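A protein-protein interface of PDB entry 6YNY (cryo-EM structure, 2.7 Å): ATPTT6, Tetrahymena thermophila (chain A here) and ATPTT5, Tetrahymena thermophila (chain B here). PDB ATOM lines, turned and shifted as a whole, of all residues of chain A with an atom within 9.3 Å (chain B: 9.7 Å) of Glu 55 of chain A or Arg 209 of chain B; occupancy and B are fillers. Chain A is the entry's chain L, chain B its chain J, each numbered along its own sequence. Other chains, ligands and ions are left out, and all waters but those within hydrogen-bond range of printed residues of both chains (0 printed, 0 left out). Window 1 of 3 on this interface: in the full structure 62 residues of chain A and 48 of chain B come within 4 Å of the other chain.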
ATOM      1  N   GLY A   6      20.848 -22.661   6.054  1.00  0.00           N
ATOM      2  CA  GLY A   6      20.253 -23.793   5.385  1.00  0.00           C
ATOM      3  C   GLY A   6      21.235 -24.446   4.441  1.00  0.00           C
ATOM      4  O   GLY A   6      22.422 -24.116   4.421  1.00  0.00           O
ATOM      5  N   GLN A   7      20.717 -25.386   3.650  1.00  0.00           N
ATOM      6  CA  GLN A   7      21.566 -26.092   2.699  1.00  0.00           C
ATOM      7  C   GLN A   7      22.052 -25.168   1.591  1.00  0.00           C
ATOM      8  O   GLN A   7      23.162 -25.349   1.077  1.00  0.00           O
ATOM      9  CB  GLN A   7      20.808 -27.275   2.103  1.00  0.00           C
ATOM     10  CG  GLN A   7      21.660 -28.195   1.249  1.00  0.00           C
ATOM     11  CD  GLN A   7      20.852 -29.297   0.597  1.00  0.00           C
ATOM     12  OE1 GLN A   7      19.632 -29.359   0.746  1.00  0.00           O
ATOM     13  NE2 GLN A   7      21.529 -30.169  -0.138  1.00  0.00           N
ATOM     14  N   ALA A   8      21.247 -24.181   1.212  1.00  0.00           N
ATOM     15  CA  ALA A   8      21.623 -23.231   0.174  1.00  0.00           C
ATOM     16  C   ALA A   8      22.533 -22.172   0.779  1.00  0.00           C
ATOM     17  O   ALA A   8      22.093 -21.362   1.601  1.00  0.00           O
ATOM     18  CB  ALA A   8      20.382 -22.598  -0.445  1.00  0.00           C
ATOM     19  N   LYS A   9      23.797 -22.175   0.378  1.00  0.00           N
ATOM     20  CA  LYS A   9      24.784 -21.251   0.907  1.00  0.00           C
ATOM     21  C   LYS A   9      25.083 -20.145  -0.097  1.00  0.00           C
ATOM     22  O   LYS A   9      24.711 -20.209  -1.269  1.00  0.00           O
ATOM     23  CB  LYS A   9      26.063 -22.000   1.278  1.00  0.00           C
ATOM     24  CG  LYS A   9      25.871 -22.960   2.432  1.00  0.00           C
ATOM     25  CD  LYS A   9      27.125 -23.745   2.734  1.00  0.00           C
ATOM     26  CE  LYS A   9      26.947 -24.576   3.991  1.00  0.00           C
ATOM     27  NZ  LYS A   9      25.756 -25.464   3.910  1.00  0.00           N
ATOM     28  N   LEU A  10      25.768 -19.116   0.390  1.00  0.00           N
ATOM     29  CA  LEU A  10      26.099 -17.959  -0.426  1.00  0.00           C
ATOM     30  C   LEU A  10      27.366 -18.242  -1.228  1.00  0.00           C
ATOM     31  O   LEU A  10      27.848 -19.375  -1.306  1.00  0.00           O
ATOM     32  CB  LEU A  10      26.238 -16.721   0.452  1.00  0.00           C
ATOM     33  CG  LEU A  10      25.004 -16.343   1.266  1.00  0.00           C
ATOM     34  CD1 LEU A  10      25.257 -15.079   2.057  1.00  0.00           C
ATOM     35  CD2 LEU A  10      23.808 -16.168   0.367  1.00  0.00           C
ATOM     36  N   GLN A  50       7.536 -16.753   0.344  1.00  0.00           N
ATOM     37  CA  GLN A  50       8.137 -17.927  -0.268  1.00  0.00           C
ATOM     38  C   GLN A  50       8.019 -17.804  -1.776  1.00  0.00           C
ATOM     39  O   GLN A  50       6.951 -17.467  -2.295  1.00  0.00           O
ATOM     40  CB  GLN A  50       7.477 -19.220   0.215  1.00  0.00           C
ATOM     41  CG  GLN A  50       8.041 -20.473  -0.426  1.00  0.00           C
ATOM     42  CD  GLN A  50       9.546 -20.586  -0.281  1.00  0.00           C
ATOM     43  OE1 GLN A  50      10.239 -21.002  -1.209  1.00  0.00           O
ATOM     44  NE2 GLN A  50      10.058 -20.221   0.887  1.00  0.00           N
ATOM     45  N   GLU A  51       9.116 -18.079  -2.470  1.00  0.00           N
ATOM     46  CA  GLU A  51       9.181 -17.927  -3.912  1.00  0.00           C
ATOM     47  C   GLU A  51       8.726 -19.208  -4.597  1.00  0.00           C
ATOM     48  O   GLU A  51       9.083 -20.312  -4.178  1.00  0.00           O
ATOM     49  CB  GLU A  51      10.608 -17.572  -4.328  1.00  0.00           C
ATOM     50  CG  GLU A  51      10.803 -17.296  -5.789  1.00  0.00           C
ATOM     51  CD  GLU A  51      12.222 -16.872  -6.100  1.00  0.00           C
ATOM     52  OE1 GLU A  51      12.786 -16.074  -5.324  1.00  0.00           O
ATOM     53  OE2 GLU A  51      12.780 -17.345  -7.111  1.00  0.00           O
ATOM     54  N   TYR A  52       7.929 -19.051  -5.648  1.00  0.00           N
ATOM     55  CA  TYR A  52       7.417 -20.181  -6.406  1.00  0.00           C
ATOM     56  C   TYR A  52       8.412 -20.592  -7.479  1.00  0.00           C
ATOM     57  O   TYR A  52       9.054 -19.747  -8.107  1.00  0.00           O
ATOM     58  CB  TYR A  52       6.073 -19.839  -7.046  1.00  0.00           C
ATOM     59  CG  TYR A  52       5.498 -20.957  -7.878  1.00  0.00           C
ATOM     60  CD1 TYR A  52       4.827 -22.011  -7.284  1.00  0.00           C
ATOM     61  CD2 TYR A  52       5.625 -20.957  -9.258  1.00  0.00           C
ATOM     62  CE1 TYR A  52       4.301 -23.036  -8.038  1.00  0.00           C
ATOM     63  CE2 TYR A  52       5.103 -21.977 -10.020  1.00  0.00           C
ATOM     64  CZ  TYR A  52       4.442 -23.015  -9.405  1.00  0.00           C
ATOM     65  OH  TYR A  52       3.919 -24.036 -10.160  1.00  0.00           O
ATOM     66  N   PHE A  53       8.535 -21.900  -7.683  1.00  0.00           N
ATOM     67  CA  PHE A  53       9.465 -22.458  -8.651  1.00  0.00           C
ATOM     68  C   PHE A  53       8.717 -23.426  -9.550  1.00  0.00           C
ATOM     69  O   PHE A  53       8.051 -24.345  -9.064  1.00  0.00           O
ATOM     70  CB  PHE A  53      10.626 -23.171  -7.960  1.00  0.00           C
ATOM     71  CG  PHE A  53      11.383 -22.305  -7.004  1.00  0.00           C
ATOM     72  CD1 PHE A  53      11.174 -22.412  -5.644  1.00  0.00           C
ATOM     73  CD2 PHE A  53      12.297 -21.376  -7.463  1.00  0.00           C
ATOM     74  CE1 PHE A  53      11.864 -21.616  -4.764  1.00  0.00           C
ATOM     75  CE2 PHE A  53      12.988 -20.578  -6.583  1.00  0.00           C
ATOM     76  CZ  PHE A  53      12.771 -20.699  -5.233  1.00  0.00           C
ATOM     77  N   LEU A  54       8.827 -23.214 -10.856  1.00  0.00           N
ATOM     78  CA  LEU A  54       8.174 -24.075 -11.831  1.00  0.00           C
ATOM     79  C   LEU A  54       8.988 -25.346 -12.019  1.00  0.00           C
ATOM     80  O   LEU A  54      10.150 -25.293 -12.434  1.00  0.00           O
ATOM     81  CB  LEU A  54       8.014 -23.338 -13.154  1.00  0.00           C
ATOM     82  CG  LEU A  54       7.347 -24.115 -14.283  1.00  0.00           C
ATOM     83  CD1 LEU A  54       5.935 -24.506 -13.903  1.00  0.00           C
ATOM     84  CD2 LEU A  54       7.354 -23.286 -15.536  1.00  0.00           C
ATOM     85  N   GLU A  55       8.377 -26.486 -11.719  1.00  0.00           N
ATOM     86  CA  GLU A  55       9.022 -27.779 -11.849  1.00  0.00           C
ATOM     87  C   GLU A  55       8.089 -28.760 -12.538  1.00  0.00           C
ATOM     88  O   GLU A  55       6.865 -28.611 -12.472  1.00  0.00           O
ATOM     89  CB  GLU A  55       9.418 -28.343 -10.479  1.00  0.00           C
ATOM     90  CG  GLU A  55      10.367 -27.469  -9.698  1.00  0.00           C
ATOM     91  CD  GLU A  55      10.758 -28.082  -8.370  1.00  0.00           C
ATOM     92  OE1 GLU A  55      10.276 -29.192  -8.062  1.00  0.00           O
ATOM     93  OE2 GLU A  55      11.548 -27.457  -7.633  1.00  0.00           O
ATOM     94  N   PRO A  56       8.637 -29.769 -13.214  1.00  0.00           N
ATOM     95  CA  PRO A  56       7.783 -30.806 -13.802  1.00  0.00           C
ATOM     96  C   PRO A  56       7.231 -31.727 -12.725  1.00  0.00           C
ATOM     97  O   PRO A  56       7.981 -32.303 -11.935  1.00  0.00           O
ATOM     98  CB  PRO A  56       8.728 -31.543 -14.754  1.00  0.00           C
ATOM     99  CG  PRO A  56      10.066 -31.326 -14.194  1.00  0.00           C
ATOM    100  CD  PRO A  56      10.053 -29.974 -13.554  1.00  0.00           C
ATOM    101  N   SER A  57       5.910 -31.861 -12.699  1.00  0.00           N
ATOM    102  CA  SER A  57       5.256 -32.678 -11.693  1.00  0.00           C
ATOM    103  C   SER A  57       5.454 -34.161 -12.000  1.00  0.00           C
ATOM    104  O   SER A  57       6.148 -34.548 -12.943  1.00  0.00           O
ATOM    105  CB  SER A  57       3.772 -32.333 -11.620  1.00  0.00           C
ATOM    106  OG  SER A  57       3.144 -32.533 -12.872  1.00  0.00           O
ATOM    107  N   GLU A  58       4.831 -35.005 -11.175  1.00  0.00           N
ATOM    108  CA  GLU A  58       4.896 -36.444 -11.402  1.00  0.00           C
ATOM    109  C   GLU A  58       4.018 -36.855 -12.575  1.00  0.00           C
ATOM    110  O   GLU A  58       4.384 -37.744 -13.350  1.00  0.00           O
ATOM    111  CB  GLU A  58       4.478 -37.191 -10.138  1.00  0.00           C
ATOM    112  CG  GLU A  58       5.184 -36.741  -8.866  1.00  0.00           C
ATOM    113  CD  GLU A  58       6.660 -37.104  -8.839  1.00  0.00           C
ATOM    114  OE1 GLU A  58       7.289 -37.161  -9.916  1.00  0.00           O
ATOM    115  OE2 GLU A  58       7.191 -37.331  -7.733  1.00  0.00           O
ATOM    116  N   LYS A  59       2.856 -36.219 -12.719  1.00  0.00           N
ATOM    117  CA  LYS A  59       2.041 -36.441 -13.906  1.00  0.00           C
ATOM    118  C   LYS A  59       2.799 -36.045 -15.161  1.00  0.00           C
ATOM    119  O   LYS A  59       2.586 -36.625 -16.232  1.00  0.00           O
ATOM    120  CB  LYS A  59       0.743 -35.645 -13.794  1.00  0.00           C
ATOM    121  CG  LYS A  59      -0.330 -36.043 -14.778  1.00  0.00           C
ATOM    122  CD  LYS A  59      -1.542 -35.140 -14.647  1.00  0.00           C
ATOM    123  CE  LYS A  59      -2.820 -35.858 -15.033  1.00  0.00           C
ATOM    124  NZ  LYS A  59      -2.730 -36.499 -16.368  1.00  0.00           N
ATOM    125  N   PHE A  60       3.686 -35.060 -15.043  1.00  0.00           N
ATOM    126  CA  PHE A  60       4.509 -34.635 -16.166  1.00  0.00           C
ATOM    127  C   PHE A  60       5.524 -35.707 -16.535  1.00  0.00           C
ATOM    128  O   PHE A  60       5.590 -36.146 -17.687  1.00  0.00           O
ATOM    129  CB  PHE A  60       5.204 -33.327 -15.802  1.00  0.00           C
ATOM    130  CG  PHE A  60       5.974 -32.702 -16.923  1.00  0.00           C
ATOM    131  CD1 PHE A  60       7.242 -33.138 -17.239  1.00  0.00           C
ATOM    132  CD2 PHE A  60       5.441 -31.648 -17.634  1.00  0.00           C
ATOM    133  CE1 PHE A  60       7.951 -32.554 -18.258  1.00  0.00           C
ATOM    134  CE2 PHE A  60       6.148 -31.061 -18.651  1.00  0.00           C
ATOM    135  CZ  PHE A  60       7.404 -31.513 -18.961  1.00  0.00           C
ATOM    136  N   LYS A  61       6.321 -36.145 -15.561  1.00  0.00           N
ATOM    137  CA  LYS A  61       7.376 -37.112 -15.826  1.00  0.00           C
ATOM    138  C   LYS A  61       6.845 -38.523 -16.025  1.00  0.00           C
ATOM    139  O   LYS A  61       7.540 -39.349 -16.625  1.00  0.00           O
ATOM    140  CB  LYS A  61       8.389 -37.104 -14.682  1.00  0.00           C
ATOM    141  CG  LYS A  61       9.029 -35.749 -14.441  1.00  0.00           C
ATOM    142  CD  LYS A  61      10.176 -35.830 -13.450  1.00  0.00           C
ATOM    143  CE  LYS A  61       9.696 -36.113 -12.043  1.00  0.00           C
ATOM    144  NZ  LYS A  61       8.882 -34.998 -11.493  1.00  0.00           N
ATOM    145  N   TRP B 204      27.640 -29.367 -11.978  1.00  0.00           N
ATOM    146  CA  TRP B 204      26.547 -28.463 -12.318  1.00  0.00           C
ATOM    147  C   TRP B 204      25.547 -28.326 -11.177  1.00  0.00           C
ATOM    148  O   TRP B 204      25.017 -27.236 -10.940  1.00  0.00           O
ATOM    149  CB  TRP B 204      25.844 -28.945 -13.586  1.00  0.00           C
ATOM    150  CG  TRP B 204      24.668 -28.113 -13.925  1.00  0.00           C
ATOM    151  CD1 TRP B 204      23.362 -28.413 -13.701  1.00  0.00           C
ATOM    152  CD2 TRP B 204      24.684 -26.821 -14.532  1.00  0.00           C
ATOM    153  NE1 TRP B 204      22.560 -27.390 -14.135  1.00  0.00           N
ATOM    154  CE2 TRP B 204      23.351 -26.399 -14.650  1.00  0.00           C
ATOM    155  CE3 TRP B 204      25.699 -25.981 -14.988  1.00  0.00           C
ATOM    156  CZ2 TRP B 204      23.006 -25.177 -15.206  1.00  0.00           C
ATOM    157  CZ3 TRP B 204      25.355 -24.771 -15.540  1.00  0.00           C
ATOM    158  CH2 TRP B 204      24.021 -24.378 -15.645  1.00  0.00           C
ATOM    159  N   ILE B 205      25.281 -29.414 -10.453  1.00  0.00           N
ATOM    160  CA  ILE B 205      24.282 -29.362  -9.391  1.00  0.00           C
ATOM    161  C   ILE B 205      24.712 -28.431  -8.266  1.00  0.00           C
ATOM    162  O   ILE B 205      23.866 -27.890  -7.545  1.00  0.00           O
ATOM    163  CB  ILE B 205      23.996 -30.774  -8.849  1.00  0.00           C
ATOM    164  CG1 ILE B 205      25.274 -31.402  -8.300  1.00  0.00           C
ATOM    165  CG2 ILE B 205      23.408 -31.648  -9.933  1.00  0.00           C
ATOM    166  CD1 ILE B 205      25.052 -32.725  -7.625  1.00  0.00           C
ATOM    167  N   HIS B 206      26.015 -28.226  -8.093  1.00  0.00           N
ATOM    168  CA  HIS B 206      26.501 -27.379  -7.011  1.00  0.00           C
ATOM    169  C   HIS B 206      26.239 -25.902  -7.248  1.00  0.00           C
ATOM    170  O   HIS B 206      26.434 -25.103  -6.326  1.00  0.00           O
ATOM    171  CB  HIS B 206      27.993 -27.611  -6.806  1.00  0.00           C
ATOM    172  CG  HIS B 206      28.320 -28.970  -6.278  1.00  0.00           C
ATOM    173  ND1 HIS B 206      28.136 -30.118  -7.017  1.00  0.00           N
ATOM    174  CD2 HIS B 206      28.806 -29.367  -5.080  1.00  0.00           C
ATOM    175  CE1 HIS B 206      28.503 -31.164  -6.298  1.00  0.00           C
ATOM    176  NE2 HIS B 206      28.914 -30.735  -5.119  1.00  0.00           N
ATOM    177  N   GLY B 207      25.815 -25.520  -8.446  1.00  0.00           N
ATOM    178  CA  GLY B 207      25.425 -24.153  -8.713  1.00  0.00           C
ATOM    179  C   GLY B 207      23.927 -23.962  -8.807  1.00  0.00           C
ATOM    180  O   GLY B 207      23.464 -22.930  -9.301  1.00  0.00           O
ATOM    181  N   THR B 208      23.157 -24.940  -8.344  1.00  0.00           N
ATOM    182  CA  THR B 208      21.710 -24.872  -8.451  1.00  0.00           C
ATOM    183  C   THR B 208      21.115 -24.261  -7.183  1.00  0.00           C
ATOM    184  O   THR B 208      21.825 -23.746  -6.316  1.00  0.00           O
ATOM    185  CB  THR B 208      21.142 -26.261  -8.726  1.00  0.00           C
ATOM    186  OG1 THR B 208      21.495 -27.144  -7.656  1.00  0.00           O
ATOM    187  CG2 THR B 208      21.694 -26.807 -10.026  1.00  0.00           C
ATOM    188  N   ARG B 209      19.788 -24.325  -7.067  1.00  0.00           N
ATOM    189  CA  ARG B 209      19.096 -23.682  -5.956  1.00  0.00           C
ATOM    190  C   ARG B 209      19.311 -24.410  -4.637  1.00  0.00           C
ATOM    191  O   ARG B 209      19.257 -23.785  -3.572  1.00  0.00           O
ATOM    192  CB  ARG B 209      17.607 -23.582  -6.280  1.00  0.00           C
ATOM    193  CG  ARG B 209      16.725 -23.222  -5.111  1.00  0.00           C
ATOM    194  CD  ARG B 209      15.360 -22.791  -5.589  1.00  0.00           C
ATOM    195  NE  ARG B 209      14.735 -23.785  -6.454  1.00  0.00           N
ATOM    196  CZ  ARG B 209      13.976 -24.785  -6.023  1.00  0.00           C
ATOM    197  NH1 ARG B 209      13.742 -24.946  -4.730  1.00  0.00           N
ATOM    198  NH2 ARG B 209      13.451 -25.633  -6.893  1.00  0.00           N
ATOM    199  N   GLN B 210      19.549 -25.720  -4.677  1.00  0.00           N
ATOM    200  CA  GLN B 210      19.696 -26.476  -3.439  1.00  0.00           C
ATOM    201  C   GLN B 210      21.023 -26.179  -2.754  1.00  0.00           C
ATOM    202  O   GLN B 210      21.097 -26.148  -1.520  1.00  0.00           O
ATOM    203  CB  GLN B 210      19.569 -27.970  -3.724  1.00  0.00           C
ATOM    204  CG  GLN B 210      18.272 -28.355  -4.406  1.00  0.00           C
ATOM    205  CD  GLN B 210      17.050 -28.008  -3.579  1.00  0.00           C
ATOM    206  OE1 GLN B 210      17.155 -27.706  -2.390  1.00  0.00           O
ATOM    207  NE2 GLN B 210      15.882 -28.045  -4.208  1.00  0.00           N
ATOM    208  N   HIS B 211      22.078 -25.956  -3.532  1.00  0.00           N
ATOM    209  CA  HIS B 211      23.408 -25.723  -2.984  1.00  0.00           C
ATOM    210  C   HIS B 211      23.832 -24.266  -3.033  1.00  0.00           C
ATOM    211  O   HIS B 211      24.537 -23.808  -2.129  1.00  0.00           O
ATOM    212  CB  HIS B 211      24.434 -26.570  -3.739  1.00  0.00           C
ATOM    213  CG  HIS B 211      24.144 -28.036  -3.705  1.00  0.00           C
ATOM    214  ND1 HIS B 211      23.193 -28.625  -4.508  1.00  0.00           N
ATOM    215  CD2 HIS B 211      24.674 -29.032  -2.958  1.00  0.00           C
ATOM    216  CE1 HIS B 211      23.153 -29.921  -4.261  1.00  0.00           C
ATOM    217  NE2 HIS B 211      24.041 -30.194  -3.324  1.00  0.00           N
ATOM    218  N   LEU B 212      23.425 -23.532  -4.063  1.00  0.00           N
ATOM    219  CA  LEU B 212      23.768 -22.126  -4.225  1.00  0.00           C
ATOM    220  C   LEU B 212      22.489 -21.312  -4.144  1.00  0.00           C
ATOM    221  O   LEU B 212      21.608 -21.448  -4.998  1.00  0.00           O
ATOM    222  CB  LEU B 212      24.480 -21.889  -5.556  1.00  0.00           C
ATOM    223  CG  LEU B 212      24.964 -20.467  -5.820  1.00  0.00           C
ATOM    224  CD1 LEU B 212      26.029 -20.083  -4.828  1.00  0.00           C
ATOM    225  CD2 LEU B 212      25.485 -20.343  -7.234  1.00  0.00           C
ATOM    226  N   ARG B 213      22.391 -20.471  -3.128  1.00  0.00           N
ATOM    227  CA  ARG B 213      21.168 -19.717  -2.910  1.00  0.00           C
ATOM    228  C   ARG B 213      21.016 -18.652  -3.988  1.00  0.00           C
ATOM    229  O   ARG B 213      21.976 -17.928  -4.272  1.00  0.00           O
ATOM    230  CB  ARG B 213      21.180 -19.064  -1.537  1.00  0.00           C
ATOM    231  CG  ARG B 213      19.801 -18.859  -0.951  1.00  0.00           C
ATOM    232  CD  ARG B 213      19.840 -17.953   0.250  1.00  0.00           C
ATOM    233  NE  ARG B 213      19.597 -16.564  -0.116  1.00  0.00           N
ATOM    234  CZ  ARG B 213      18.399 -15.989  -0.107  1.00  0.00           C
ATOM    235  NH1 ARG B 213      17.323 -16.671   0.251  1.00  0.00           N
ATOM    236  NH2 ARG B 213      18.278 -14.720  -0.458  1.00  0.00           N
ATOM    237  N   PRO B 214      19.846 -18.520  -4.606  1.00  0.00           N
ATOM    238  CA  PRO B 214      19.647 -17.435  -5.570  1.00  0.00           C
ATOM    239  C   PRO B 214      19.726 -16.075  -4.896  1.00  0.00           C
ATOM    240  O   PRO B 214      19.754 -15.947  -3.671  1.00  0.00           O
ATOM    241  CB  PRO B 214      18.251 -17.704  -6.133  1.00  0.00           C
ATOM    242  CG  PRO B 214      17.963 -19.111  -5.810  1.00  0.00           C
ATOM    243  CD  PRO B 214      18.678 -19.412  -4.549  1.00  0.00           C
ATOM    244  N   ASP B 215      19.763 -15.040  -5.727  1.00  0.00           N
ATOM    245  CA  ASP B 215      19.822 -13.660  -5.251  1.00  0.00           C
ATOM    246  C   ASP B 215      18.424 -13.085  -5.043  1.00  0.00           C
ATOM    247  O   ASP B 215      18.077 -12.028  -5.565  1.00  0.00           O
ATOM    248  CB  ASP B 215      20.623 -12.810  -6.227  1.00  0.00           C
ATOM    249  CG  ASP B 215      20.963 -11.447  -5.670  1.00  0.00           C
ATOM    250  OD1 ASP B 215      20.587 -11.166  -4.513  1.00  0.00           O
ATOM    251  OD2 ASP B 215      21.607 -10.654  -6.386  1.00  0.00           O
ATOM    252  N   THR B 216      17.607 -13.798  -4.272  1.00  0.00           N
ATOM    253  CA  THR B 216      16.273 -13.344  -3.913  1.00  0.00           C
ATOM    254  C   THR B 216      16.033 -13.641  -2.442  1.00  0.00           C
ATOM    255  O   THR B 216      16.583 -14.597  -1.889  1.00  0.00           O
ATOM    256  CB  THR B 216      15.196 -14.014  -4.772  1.00  0.00           C
ATOM    257  OG1 THR B 216      15.313 -15.436  -4.674  1.00  0.00           O
ATOM    258  CG2 THR B 216      15.344 -13.601  -6.219  1.00  0.00           C
ATOM    259  N   TRP B 218      13.156 -14.440  -0.809  1.00  0.00           N
ATOM    260  CA  TRP B 218      12.190 -15.474  -0.465  1.00  0.00           C
ATOM    261  C   TRP B 218      12.445 -16.775  -1.212  1.00  0.00           C
ATOM    262  O   TRP B 218      11.521 -17.569  -1.404  1.00  0.00           O
ATOM    263  CB  TRP B 218      10.770 -14.977  -0.725  1.00  0.00           C
ATOM    264  CG  TRP B 218      10.478 -13.668  -0.080  1.00  0.00           C
ATOM    265  CD1 TRP B 218       9.916 -12.577  -0.666  1.00  0.00           C
ATOM    266  CD2 TRP B 218      10.747 -13.300   1.276  1.00  0.00           C
ATOM    267  NE1 TRP B 218       9.812 -11.553   0.240  1.00  0.00           N
ATOM    268  CE2 TRP B 218      10.314 -11.974   1.442  1.00  0.00           C
ATOM    269  CE3 TRP B 218      11.308 -13.965   2.369  1.00  0.00           C
ATOM    270  CZ2 TRP B 218      10.427 -11.300   2.652  1.00  0.00           C
ATOM    271  CZ3 TRP B 218      11.415 -13.295   3.565  1.00  0.00           C
ATOM    272  CH2 TRP B 218      10.979 -11.978   3.698  1.00  0.00           C
ATOM    273  N   ALA B 219      13.687 -17.010  -1.637  1.00  0.00           N
ATOM    274  CA  ALA B 219      14.030 -18.290  -2.240  1.00  0.00           C
ATOM    275  C   ALA B 219      14.004 -19.411  -1.213  1.00  0.00           C
ATOM    276  O   ALA B 219      13.650 -20.548  -1.545  1.00  0.00           O
ATOM    277  CB  ALA B 219      15.406 -18.209  -2.892  1.00  0.00           C
ATOM    278  N   ASP B 220      14.372 -19.113   0.028  1.00  0.00           N
ATOM    279  CA  ASP B 220      14.356 -20.083   1.110  1.00  0.00           C
ATOM    280  C   ASP B 220      13.915 -19.364   2.380  1.00  0.00           C
ATOM    281  O   ASP B 220      13.423 -18.232   2.338  1.00  0.00           O
ATOM    282  CB  ASP B 220      15.727 -20.755   1.252  1.00  0.00           C
ATOM    283  CG  ASP B 220      16.840 -19.760   1.506  1.00  0.00           C
ATOM    284  OD1 ASP B 220      16.567 -18.542   1.497  1.00  0.00           O
ATOM    285  OD2 ASP B 220      17.990 -20.197   1.713  1.00  0.00           O
ATOM    286  N   ASP B 221      14.094 -20.027   3.523  1.00  0.00           N
ATOM    287  CA  ASP B 221      13.679 -19.502   4.817  1.00  0.00           C
ATOM    288  C   ASP B 221      14.797 -18.757   5.538  1.00  0.00           C
ATOM    289  O   ASP B 221      14.866 -18.792   6.774  1.00  0.00           O
ATOM    290  CB  ASP B 221      13.146 -20.638   5.691  1.00  0.00           C
ATOM    291  CG  ASP B 221      14.102 -21.810   5.773  1.00  0.00           C
ATOM    292  OD1 ASP B 221      15.266 -21.606   6.177  1.00  0.00           O
ATOM    293  OD2 ASP B 221      13.690 -22.937   5.431  1.00  0.00           O
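The side-chain carboxylate (OE2) of Glu 55 of chain A is in salt-bridge range of the guanidinium group (NH2) of Arg 209 of chain B (2.7 Å).
The backbone carbonyl oxygen of Gln 210 of chain B is in hydrogen-bond range of the backbone NH of Ala 8 of chain A.
The backbone carbonyl oxygen of His 211 of chain B is in hydrogen-bond range of the backbone NH of Lys 9 of chain A (3.1 Å).
The backbone NH (N) of Arg 213 of chain B sits at hydrogen-bond distance from the backbone carbonyl oxygen (O) of Lys 9 of chain A (3.0 Å).
The side-chain carboxylate of Glu 51 of chain A is in hydrogen-bond range of the side-chain hydroxyl of Thr 216 of chain B, 2.7 Å away.
N of Glu 51 of chain A sits at hydrogen-bond distance from O of Trp 218 of chain B (2.7 Å).
The backbone carbonyl oxygen (O) of Ala 219 of chain B sits close to the side-chain amide oxygen (OE1) of Gln 50 of chain A (3.5 Å).
The backbone carbonyl oxygen (O) of Gln 210 of chain B lies close to the backbone carbonyl oxygen (O) of Gln 7 of chain A, 3.4 Å away.
The backbone carbonyl oxygen (O) of Ile 205 of chain B is in hydrogen-bond range of a ring nitrogen (ND1) of His 211 of chain B, at 3.2 Å.
The guanidinium group (NH1) of Arg 213 of chain B sits close to the backbone carbonyl oxygen (O) of Thr 216 of chain B (3.1 Å).
The guanidinium group of Arg 213 of chain B is in salt-bridge range of the side-chain carboxylate of Asp 220 of chain B (3.9 Å).
Gln 7 of chain A touches His 211 of chain B.
Ala 8 of chain A touches Arg 209 of chain B (CB to O, 3.5 Å).
His 211 of chain B touches Ala 8 of chain A.
Arg 213 of chain B touches Ala 8 of chain A (CB to CB, 3.8 Å).
Lys 9 of chain A touches Leu 212 of chain B (O to CA, 3.6 Å).
Gln 50 of chain A touches Trp 218 of chain B.
Glu 51 of chain A touches Ala 219 of chain B.
Phe 53 of chain A touches Arg 209 of chain B.
Phe 53 of chain A touches Ala 219 of chain B (CZ to O, 3.8 Å).
Of chain B, only Arg 209 (2.7 Å) comes within 4 Å of Glu 55 of chain A.
Of chain A, only Ala 8 (3.5 Å), Phe 53 (3.3 Å) and Glu 55 (2.7 Å) come within 4 Å of Arg 209 of chain B.
No residue of chain B comes within 4 Å of Leu 54 of chain A.
No residue of chain B comes within 4 Å of Pro 56 of chain A.
No residue of chain A comes within 4 Å of Thr 208 of chain B.
Gln 210 of chain B touches just these residues of chain A: Gln 7 (3.4 Å) and Ala 8 (3.4 Å).
Printed residues of chain A within 4 Å of His 211 of chain B: Gln 7, Ala 8 and Lys 9.
Of the printed residues of chain B, Phe 53 of chain A touches Arg 209 and Ala 219.
Of the printed residues of chain B, Gln 50 of chain A touches Trp 218 and Ala 219.
Of the printed residues of chain B, Ala 8 of chain A touches Arg 209, Gln 210, His 211 and Arg 213.
Printed residues of chain B within 4 Å of Gln 7 of chain A: Gln 210 (3.4 Å) and His 211 (3.8 Å).
Asp 220 of chain B touches none of the printed residues of chain A.
The nearest residue of chain B that does not touch Glu 55 of chain A is Gln 210 of chain B (5.6 Å).
The nearest residue of chain A that does not touch Arg 209 of chain B is Gln 7 of chain A (6.0 Å).
The nearest printed residue of chain B that does not touch Gln 7 of chain A is Leu 212 of chain B (5.5 Å).
Of the 17 printed residues of chain B, 8 touch a printed residue of chain A.
Hydrophobic or aromatic side chains of chain B that line the printed part of chain A: Leu 212 and Trp 218.
Among the printed residues, 17 pairs touch across the chains.
Among the printed residues, Asp or Glu carboxylates within 4 Å of a Lys or Arg side-chain nitrogen of the other chain: Glu 55 of chain A with Arg 209 of chain B (2.7 Å).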
